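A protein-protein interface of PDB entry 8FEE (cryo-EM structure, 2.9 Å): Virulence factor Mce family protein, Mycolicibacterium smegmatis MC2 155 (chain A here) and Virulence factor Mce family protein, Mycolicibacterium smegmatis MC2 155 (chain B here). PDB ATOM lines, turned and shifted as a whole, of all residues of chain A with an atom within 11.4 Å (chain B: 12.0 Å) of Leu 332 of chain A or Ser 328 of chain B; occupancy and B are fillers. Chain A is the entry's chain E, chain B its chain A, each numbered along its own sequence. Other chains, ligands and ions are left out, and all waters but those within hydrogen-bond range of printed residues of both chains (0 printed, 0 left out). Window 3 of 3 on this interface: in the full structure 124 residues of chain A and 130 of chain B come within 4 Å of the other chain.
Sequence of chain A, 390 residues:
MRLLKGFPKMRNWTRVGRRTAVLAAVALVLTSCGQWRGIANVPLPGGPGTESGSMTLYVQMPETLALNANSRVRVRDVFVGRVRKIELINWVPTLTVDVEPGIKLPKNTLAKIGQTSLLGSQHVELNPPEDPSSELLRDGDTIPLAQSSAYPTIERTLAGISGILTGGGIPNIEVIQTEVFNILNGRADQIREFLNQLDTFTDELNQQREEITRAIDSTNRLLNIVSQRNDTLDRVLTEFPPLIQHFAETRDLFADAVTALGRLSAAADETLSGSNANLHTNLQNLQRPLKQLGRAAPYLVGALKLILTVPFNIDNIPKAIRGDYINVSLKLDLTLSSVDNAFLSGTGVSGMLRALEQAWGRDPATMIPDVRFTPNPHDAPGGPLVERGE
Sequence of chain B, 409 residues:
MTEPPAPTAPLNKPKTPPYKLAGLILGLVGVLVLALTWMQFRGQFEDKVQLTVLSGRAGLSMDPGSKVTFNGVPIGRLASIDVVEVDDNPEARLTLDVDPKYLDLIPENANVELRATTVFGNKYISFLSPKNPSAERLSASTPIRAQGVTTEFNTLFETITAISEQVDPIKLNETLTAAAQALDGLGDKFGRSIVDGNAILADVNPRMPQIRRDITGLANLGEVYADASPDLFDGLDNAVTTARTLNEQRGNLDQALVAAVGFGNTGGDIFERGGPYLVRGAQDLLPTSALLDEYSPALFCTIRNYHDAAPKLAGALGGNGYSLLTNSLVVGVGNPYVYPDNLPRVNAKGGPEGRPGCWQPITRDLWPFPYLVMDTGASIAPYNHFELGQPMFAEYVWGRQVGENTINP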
ATOM      1  N   ASN A 327     -24.244 -10.522 -22.768  1.00  0.00           N
ATOM      2  CA  ASN A 327     -23.605 -11.366 -21.765  1.00  0.00           C
ATOM      3  C   ASN A 327     -22.129 -11.006 -21.649  1.00  0.00           C
ATOM      4  O   ASN A 327     -21.393 -11.047 -22.641  1.00  0.00           O
ATOM      5  CB  ASN A 327     -23.774 -12.840 -22.122  1.00  0.00           C
ATOM      6  CG  ASN A 327     -25.219 -13.292 -22.064  1.00  0.00           C
ATOM      7  OD1 ASN A 327     -26.055 -12.660 -21.419  1.00  0.00           O
ATOM      8  ND2 ASN A 327     -25.520 -14.396 -22.734  1.00  0.00           N
ATOM      9  N   VAL A 328     -21.695 -10.659 -20.438  1.00  0.00           N
ATOM     10  CA  VAL A 328     -20.331 -10.212 -20.181  1.00  0.00           C
ATOM     11  C   VAL A 328     -19.798 -10.952 -18.959  1.00  0.00           C
ATOM     12  O   VAL A 328     -20.546 -11.241 -18.018  1.00  0.00           O
ATOM     13  CB  VAL A 328     -20.261  -8.678 -19.994  1.00  0.00           C
ATOM     14  CG1 VAL A 328     -20.987  -8.237 -18.728  1.00  0.00           C
ATOM     15  CG2 VAL A 328     -18.817  -8.193 -19.997  1.00  0.00           C
ATOM     16  N   SER A 329     -18.514 -11.300 -18.997  1.00  0.00           N
ATOM     17  CA  SER A 329     -17.843 -11.982 -17.896  1.00  0.00           C
ATOM     18  C   SER A 329     -16.935 -10.987 -17.185  1.00  0.00           C
ATOM     19  O   SER A 329     -15.999 -10.452 -17.791  1.00  0.00           O
ATOM     20  CB  SER A 329     -17.043 -13.182 -18.401  1.00  0.00           C
ATOM     21  OG  SER A 329     -16.131 -12.791 -19.410  1.00  0.00           O
ATOM     22  N   LEU A 330     -17.206 -10.750 -15.906  1.00  0.00           N
ATOM     23  CA  LEU A 330     -16.587  -9.665 -15.153  1.00  0.00           C
ATOM     24  C   LEU A 330     -15.423 -10.205 -14.333  1.00  0.00           C
ATOM     25  O   LEU A 330     -15.607 -11.090 -13.491  1.00  0.00           O
ATOM     26  CB  LEU A 330     -17.612  -8.987 -14.244  1.00  0.00           C
ATOM     27  CG  LEU A 330     -18.827  -8.380 -14.944  1.00  0.00           C
ATOM     28  CD1 LEU A 330     -19.792  -7.788 -13.928  1.00  0.00           C
ATOM     29  CD2 LEU A 330     -18.390  -7.329 -15.952  1.00  0.00           C
ATOM     30  N   LYS A 331     -14.232  -9.667 -14.576  1.00  0.00           N
ATOM     31  CA  LYS A 331     -13.039  -9.953 -13.784  1.00  0.00           C
ATOM     32  C   LYS A 331     -12.730  -8.688 -12.985  1.00  0.00           C
ATOM     33  O   LYS A 331     -11.990  -7.813 -13.435  1.00  0.00           O
ATOM     34  CB  LYS A 331     -11.866 -10.366 -14.678  1.00  0.00           C
ATOM     35  CG  LYS A 331     -10.536 -10.518 -13.954  1.00  0.00           C
ATOM     36  CD  LYS A 331     -10.162 -11.972 -13.755  1.00  0.00           C
ATOM     37  CE  LYS A 331      -9.686 -12.597 -15.053  1.00  0.00           C
ATOM     38  NZ  LYS A 331      -9.136 -13.965 -14.840  1.00  0.00           N
ATOM     39  N   LEU A 332     -13.333  -8.583 -11.800  1.00  0.00           N
ATOM     40  CA  LEU A 332     -13.118  -7.432 -10.923  1.00  0.00           C
ATOM     41  C   LEU A 332     -11.724  -7.539 -10.312  1.00  0.00           C
ATOM     42  O   LEU A 332     -11.531  -8.032  -9.198  1.00  0.00           O
ATOM     43  CB  LEU A 332     -14.189  -7.354  -9.840  1.00  0.00           C
ATOM     44  CG  LEU A 332     -15.619  -6.947 -10.210  1.00  0.00           C
ATOM     45  CD1 LEU A 332     -16.400  -8.096 -10.834  1.00  0.00           C
ATOM     46  CD2 LEU A 332     -16.346  -6.405  -8.990  1.00  0.00           C
ATOM     47  N   ASP A 333     -10.732  -7.059 -11.056  1.00  0.00           N
ATOM     48  CA  ASP A 333      -9.344  -7.245 -10.655  1.00  0.00           C
ATOM     49  C   ASP A 333      -8.948  -6.162  -9.656  1.00  0.00           C
ATOM     50  O   ASP A 333      -8.994  -4.967  -9.965  1.00  0.00           O
ATOM     51  CB  ASP A 333      -8.422  -7.253 -11.875  1.00  0.00           C
ATOM     52  CG  ASP A 333      -8.476  -5.964 -12.663  1.00  0.00           C
ATOM     53  OD1 ASP A 333      -9.579  -5.398 -12.798  1.00  0.00           O
ATOM     54  OD2 ASP A 333      -7.414  -5.517 -13.143  1.00  0.00           O
ATOM     55  N   LEU A 334      -8.589  -6.583  -8.446  1.00  0.00           N
ATOM     56  CA  LEU A 334      -8.127  -5.691  -7.390  1.00  0.00           C
ATOM     57  C   LEU A 334      -6.622  -5.820  -7.176  1.00  0.00           C
ATOM     58  O   LEU A 334      -6.126  -5.733  -6.051  1.00  0.00           O
ATOM     59  CB  LEU A 334      -8.883  -5.959  -6.092  1.00  0.00           C
ATOM     60  CG  LEU A 334     -10.406  -6.043  -6.216  1.00  0.00           C
ATOM     61  CD1 LEU A 334     -11.045  -6.278  -4.859  1.00  0.00           C
ATOM     62  CD2 LEU A 334     -10.962  -4.784  -6.860  1.00  0.00           C
ATOM     63  N   THR A 335      -5.883  -6.039  -8.259  1.00  0.00           N
ATOM     64  CA  THR A 335      -4.433  -6.120  -8.188  1.00  0.00           C
ATOM     65  C   THR A 335      -3.849  -4.768  -7.775  1.00  0.00           C
ATOM     66  O   THR A 335      -4.461  -3.713  -7.967  1.00  0.00           O
ATOM     67  CB  THR A 335      -3.868  -6.558  -9.543  1.00  0.00           C
ATOM     68  OG1 THR A 335      -4.721  -7.558 -10.111  1.00  0.00           O
ATOM     69  CG2 THR A 335      -2.474  -7.145  -9.395  1.00  0.00           C
ATOM     70  N   LEU A 336      -2.652  -4.813  -7.180  1.00  0.00           N
ATOM     71  CA  LEU A 336      -2.002  -3.585  -6.731  1.00  0.00           C
ATOM     72  C   LEU A 336      -1.693  -2.661  -7.903  1.00  0.00           C
ATOM     73  O   LEU A 336      -1.904  -1.447  -7.816  1.00  0.00           O
ATOM     74  CB  LEU A 336      -0.726  -3.910  -5.953  1.00  0.00           C
ATOM     75  CG  LEU A 336      -0.895  -4.474  -4.542  1.00  0.00           C
ATOM     76  CD1 LEU A 336       0.452  -4.584  -3.847  1.00  0.00           C
ATOM     77  CD2 LEU A 336      -1.857  -3.625  -3.724  1.00  0.00           C
ATOM     78  N   SER A 337      -1.187  -3.218  -9.007  1.00  0.00           N
ATOM     79  CA  SER A 337      -0.861  -2.396 -10.169  1.00  0.00           C
ATOM     80  C   SER A 337      -2.115  -1.806 -10.803  1.00  0.00           C
ATOM     81  O   SER A 337      -2.104  -0.658 -11.264  1.00  0.00           O
ATOM     82  CB  SER A 337      -0.083  -3.219 -11.193  1.00  0.00           C
ATOM     83  OG  SER A 337      -0.864  -4.294 -11.681  1.00  0.00           O
ATOM     84  N   SER A 338      -3.202  -2.582 -10.847  1.00  0.00           N
ATOM     85  CA  SER A 338      -4.449  -2.082 -11.414  1.00  0.00           C
ATOM     86  C   SER A 338      -4.999  -0.915 -10.602  1.00  0.00           C
ATOM     87  O   SER A 338      -5.446   0.089 -11.170  1.00  0.00           O
ATOM     88  CB  SER A 338      -5.478  -3.209 -11.496  1.00  0.00           C
ATOM     89  OG  SER A 338      -5.846  -3.657 -10.204  1.00  0.00           O
ATOM     90  N   VAL A 339      -4.971  -1.026  -9.273  1.00  0.00           N
ATOM     91  CA  VAL A 339      -5.443   0.064  -8.423  1.00  0.00           C
ATOM     92  C   VAL A 339      -4.496   1.258  -8.509  1.00  0.00           C
ATOM     93  O   VAL A 339      -4.930   2.416  -8.475  1.00  0.00           O
ATOM     94  CB  VAL A 339      -5.615  -0.436  -6.976  1.00  0.00           C
ATOM     95  CG1 VAL A 339      -5.855   0.720  -6.017  1.00  0.00           C
ATOM     96  CG2 VAL A 339      -6.761  -1.432  -6.901  1.00  0.00           C
ATOM     97  N   ASN A 341      -2.751   2.178 -11.180  1.00  0.00           N
ATOM     98  CA  ASN A 341      -3.055   2.883 -12.420  1.00  0.00           C
ATOM     99  C   ASN A 341      -4.428   3.538 -12.378  1.00  0.00           C
ATOM    100  O   ASN A 341      -4.630   4.590 -12.995  1.00  0.00           O
ATOM    101  CB  ASN A 341      -2.956   1.931 -13.612  1.00  0.00           C
ATOM    102  CG  ASN A 341      -1.571   1.916 -14.228  1.00  0.00           C
ATOM    103  OD1 ASN A 341      -0.724   2.745 -13.898  1.00  0.00           O
ATOM    104  ND2 ASN A 341      -1.336   0.973 -15.131  1.00  0.00           N
ATOM    105  N   ALA A 342      -5.379   2.941 -11.659  1.00  0.00           N
ATOM    106  CA  ALA A 342      -6.741   3.468 -11.649  1.00  0.00           C
ATOM    107  C   ALA A 342      -6.855   4.732 -10.807  1.00  0.00           C
ATOM    108  O   ALA A 342      -7.567   5.670 -11.186  1.00  0.00           O
ATOM    109  CB  ALA A 342      -7.709   2.402 -11.138  1.00  0.00           C
ATOM    110  N   PHE A 343      -6.171   4.781  -9.665  1.00  0.00           N
ATOM    111  CA  PHE A 343      -6.315   5.887  -8.725  1.00  0.00           C
ATOM    112  C   PHE A 343      -5.072   6.763  -8.643  1.00  0.00           C
ATOM    113  O   PHE A 343      -5.155   7.976  -8.852  1.00  0.00           O
ATOM    114  CB  PHE A 343      -6.672   5.344  -7.334  1.00  0.00           C
ATOM    115  CG  PHE A 343      -8.098   4.892  -7.206  1.00  0.00           C
ATOM    116  CD1 PHE A 343      -9.136   5.807  -7.272  1.00  0.00           C
ATOM    117  CD2 PHE A 343      -8.402   3.556  -7.009  1.00  0.00           C
ATOM    118  CE1 PHE A 343     -10.450   5.395  -7.151  1.00  0.00           C
ATOM    119  CE2 PHE A 343      -9.714   3.138  -6.886  1.00  0.00           C
ATOM    120  CZ  PHE A 343     -10.739   4.060  -6.958  1.00  0.00           C
ATOM    121  N   ILE A 368       0.503  -4.545 -16.051  1.00  0.00           N
ATOM    122  CA  ILE A 368       0.111  -3.457 -16.953  1.00  0.00           C
ATOM    123  C   ILE A 368       1.196  -2.383 -16.931  1.00  0.00           C
ATOM    124  O   ILE A 368       1.668  -2.007 -15.839  1.00  0.00           O
ATOM    125  CB  ILE A 368      -1.265  -2.891 -16.539  1.00  0.00           C
ATOM    126  CG1 ILE A 368      -1.631  -1.637 -17.334  1.00  0.00           C
ATOM    127  CG2 ILE A 368      -1.330  -2.637 -15.038  1.00  0.00           C
ATOM    128  CD1 ILE A 368      -3.047  -1.170 -17.098  1.00  0.00           C
ATOM    129  N   LEU B 324     -18.292 -12.321 -23.143  1.00  0.00           N
ATOM    130  CA  LEU B 324     -17.144 -11.474 -23.430  1.00  0.00           C
ATOM    131  C   LEU B 324     -16.210 -11.446 -22.229  1.00  0.00           C
ATOM    132  O   LEU B 324     -16.657 -11.332 -21.084  1.00  0.00           O
ATOM    133  CB  LEU B 324     -17.585 -10.053 -23.787  1.00  0.00           C
ATOM    134  CG  LEU B 324     -17.078  -9.530 -25.130  1.00  0.00           C
ATOM    135  CD1 LEU B 324     -17.799  -8.251 -25.514  1.00  0.00           C
ATOM    136  CD2 LEU B 324     -15.577  -9.304 -25.074  1.00  0.00           C
ATOM    137  N   LEU B 325     -14.911 -11.545 -22.498  1.00  0.00           N
ATOM    138  CA  LEU B 325     -13.885 -11.574 -21.464  1.00  0.00           C
ATOM    139  C   LEU B 325     -13.318 -10.173 -21.280  1.00  0.00           C
ATOM    140  O   LEU B 325     -12.692  -9.630 -22.196  1.00  0.00           O
ATOM    141  CB  LEU B 325     -12.770 -12.552 -21.830  1.00  0.00           C
ATOM    142  CG  LEU B 325     -13.128 -14.030 -21.964  1.00  0.00           C
ATOM    143  CD1 LEU B 325     -11.941 -14.802 -22.512  1.00  0.00           C
ATOM    144  CD2 LEU B 325     -13.544 -14.579 -20.614  1.00  0.00           C
ATOM    145  N   THR B 326     -13.530  -9.595 -20.098  1.00  0.00           N
ATOM    146  CA  THR B 326     -13.067  -8.245 -19.817  1.00  0.00           C
ATOM    147  C   THR B 326     -12.499  -8.165 -18.408  1.00  0.00           C
ATOM    148  O   THR B 326     -12.897  -8.915 -17.514  1.00  0.00           O
ATOM    149  CB  THR B 326     -14.198  -7.211 -19.957  1.00  0.00           C
ATOM    150  OG1 THR B 326     -15.337  -7.640 -19.199  1.00  0.00           O
ATOM    151  CG2 THR B 326     -14.599  -7.028 -21.414  1.00  0.00           C
ATOM    152  N   ASN B 327     -11.561  -7.237 -18.223  1.00  0.00           N
ATOM    153  CA  ASN B 327     -11.028  -6.888 -16.911  1.00  0.00           C
ATOM    154  C   ASN B 327     -11.721  -5.621 -16.434  1.00  0.00           C
ATOM    155  O   ASN B 327     -11.664  -4.590 -17.112  1.00  0.00           O
ATOM    156  CB  ASN B 327      -9.516  -6.675 -16.970  1.00  0.00           C
ATOM    157  CG  ASN B 327      -8.767  -7.916 -17.392  1.00  0.00           C
ATOM    158  OD1 ASN B 327      -9.180  -9.033 -17.090  1.00  0.00           O
ATOM    159  ND2 ASN B 327      -7.656  -7.729 -18.097  1.00  0.00           N
ATOM    160  N   SER B 328     -12.360  -5.688 -15.272  1.00  0.00           N
ATOM    161  CA  SER B 328     -13.077  -4.544 -14.715  1.00  0.00           C
ATOM    162  C   SER B 328     -12.368  -4.084 -13.448  1.00  0.00           C
ATOM    163  O   SER B 328     -12.508  -4.700 -12.389  1.00  0.00           O
ATOM    164  CB  SER B 328     -14.534  -4.902 -14.434  1.00  0.00           C
ATOM    165  OG  SER B 328     -15.259  -5.072 -15.638  1.00  0.00           O
ATOM    166  N   LEU B 329     -11.618  -2.994 -13.552  1.00  0.00           N
ATOM    167  CA  LEU B 329     -11.006  -2.349 -12.400  1.00  0.00           C
ATOM    168  C   LEU B 329     -11.731  -1.039 -12.132  1.00  0.00           C
ATOM    169  O   LEU B 329     -12.021  -0.287 -13.065  1.00  0.00           O
ATOM    170  CB  LEU B 329      -9.506  -2.125 -12.626  1.00  0.00           C
ATOM    171  CG  LEU B 329      -8.994  -1.422 -13.889  1.00  0.00           C
ATOM    172  CD1 LEU B 329      -8.895   0.083 -13.711  1.00  0.00           C
ATOM    173  CD2 LEU B 329      -7.650  -1.997 -14.312  1.00  0.00           C
ATOM    174  N   VAL B 330     -12.058  -0.789 -10.863  1.00  0.00           N
ATOM    175  CA  VAL B 330     -12.836   0.393 -10.514  1.00  0.00           C
ATOM    176  C   VAL B 330     -12.025   1.650 -10.804  1.00  0.00           C
ATOM    177  O   VAL B 330     -10.824   1.721 -10.514  1.00  0.00           O
ATOM    178  CB  VAL B 330     -13.277   0.333  -9.041  1.00  0.00           C
ATOM    179  CG1 VAL B 330     -14.406  -0.672  -8.872  1.00  0.00           C
ATOM    180  CG2 VAL B 330     -12.106  -0.034  -8.146  1.00  0.00           C
ATOM    181  N   VAL B 331     -12.681   2.650 -11.396  1.00  0.00           N
ATOM    182  CA  VAL B 331     -12.038   3.908 -11.749  1.00  0.00           C
ATOM    183  C   VAL B 331     -13.069   5.005 -11.504  1.00  0.00           C
ATOM    184  O   VAL B 331     -14.268   4.742 -11.391  1.00  0.00           O
ATOM    185  CB  VAL B 331     -11.532   3.905 -13.220  1.00  0.00           C
ATOM    186  CG1 VAL B 331     -12.682   3.784 -14.204  1.00  0.00           C
ATOM    187  CG2 VAL B 331     -10.610   5.076 -13.538  1.00  0.00           C
ATOM    188  N   GLY B 332     -12.596   6.243 -11.417  1.00  0.00           N
ATOM    189  CA  GLY B 332     -13.467   7.395 -11.240  1.00  0.00           C
ATOM    190  C   GLY B 332     -13.775   8.065 -12.568  1.00  0.00           C
ATOM    191  O   GLY B 332     -12.915   8.158 -13.444  1.00  0.00           O
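The backbone carbonyl oxygen (O) of Thr 335 of chain A sits at hydrogen-bond distance from the side-chain hydroxyl (OG) of Ser 338 of chain A, 2.6 Å away. OG of Ser 338 of chain A is in hydrogen-bond range of O of Asp 333 of chain A (3.4 Å).
Printed residues of chain B within 4 Å of Asn 327 of chain A: Leu 324. Printed residues of chain B within 4 Å of Val 328 of chain A: Leu 324 (3.8 Å) and Thr 326 (3.6 Å). Of chain B, only Ser 328 (3.9 Å) comes within 4 Å of Leu 330 of chain A. Leu 332 of chain A touches just one residue of chain B: Ser 328. Of chain B, only Ser 328 and Leu 329 come within 4 Å of Asp 333 of chain A. Printed residues of chain B within 4 Å of Ser 338 of chain A: Leu 329. Printed residues of chain A within 4 Å of Leu 325 of chain B: Ser 329 (3.3 Å). Of chain A, only Lys 331 comes within 4 Å of Asn 327 of chain B. Ser 328 of chain B touches just these residues of chain A: Leu 330, Lys 331, Leu 332 and Asp 333. Leu 329 of chain B touches three residues of chain A. Val 330 of chain B touches just one residue of chain A: Ala 342. Gly 332 of chain B touches none of the printed residues of chain A. The nearest residue of chain B that does not touch Leu 332 of chain A is Leu 329 of chain B (5.4 Å). The nearest residue of chain A that does not touch Ser 328 of chain B is Leu 334 of chain A (5.7 Å). The nearest printed residue of chain B that does not touch Ser 329 of chain A is Asn 327 of chain B (5.5 Å).
Val 328 of chain A touches Leu 324 of chain B. OG1 of Thr 326 of chain B touches CG2 of Val 328 of chain A, 3.6 Å away. OG of Ser 329 of chain A touches CA of Leu 325 of chain B (3.3 Å). CD2 of Leu 330 of chain A touches OG of Ser 328 of chain B, at 3.9 Å. Asn 327 of chain B touches Lys 331 of chain A. Ser 328 of chain B touches Leu 332 of chain A (O to CA, 3.2 Å). Ser 338 of chain A touches Leu 329 of chain B (CB to CD2, 3.8 Å). Ala 342 of chain A touches Leu 329 of chain B. Val 330 of chain B touches Ala 342 of chain A. O of Ala 342 of chain A touches CG2 of Val 331 of chain B, at 3.9 Å.
The backbone carbonyl oxygen (O) of Thr 326 of chain B lies within hydrogen-bond range of the backbone NH (N) of Lys 331 of chain A. The backbone carbonyl oxygen (O) of Asn 327 of chain A is in hydrogen-bond range of the backbone NH (N) of Leu 324 of chain B (3.4 Å). The backbone carbonyl oxygen (O) of Leu 324 of chain B lies within hydrogen-bond range of the backbone NH (N) of Ser 329 of chain A, 2.8 Å away. N of Asp 333 of chain A sits at hydrogen-bond distance from O of Ser 328 of chain B (3.2 Å). OG1 of Thr 326 of chain B sits at hydrogen-bond distance from O of Ser 329 of chain A. The side-chain carboxylate (OD1) of Asp 333 of chain A lies within hydrogen-bond range of the backbone NH (N) of Leu 329 of chain B (3.2 Å). The backbone carbonyl oxygen (O) of Lys 331 of chain A lies within hydrogen-bond range of the backbone NH (N) of Ser 328 of chain B.
Of the 17 printed residues of chain A, 9 touch a printed residue of chain B. Hydrophobic or aromatic side chains of chain A within 4 Å of the printed part of chain B: Val 328, Leu 330 and Ala 342. Along chain A the printed residues that touch a printed residue of chain B span positions 327 to 342. Among the printed residues, 17 pairs touch across the chains. Among the printed residues, no Asp or Glu carboxylate lies within 4 Å of a Lys or Arg side-chain nitrogen of the other chain.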
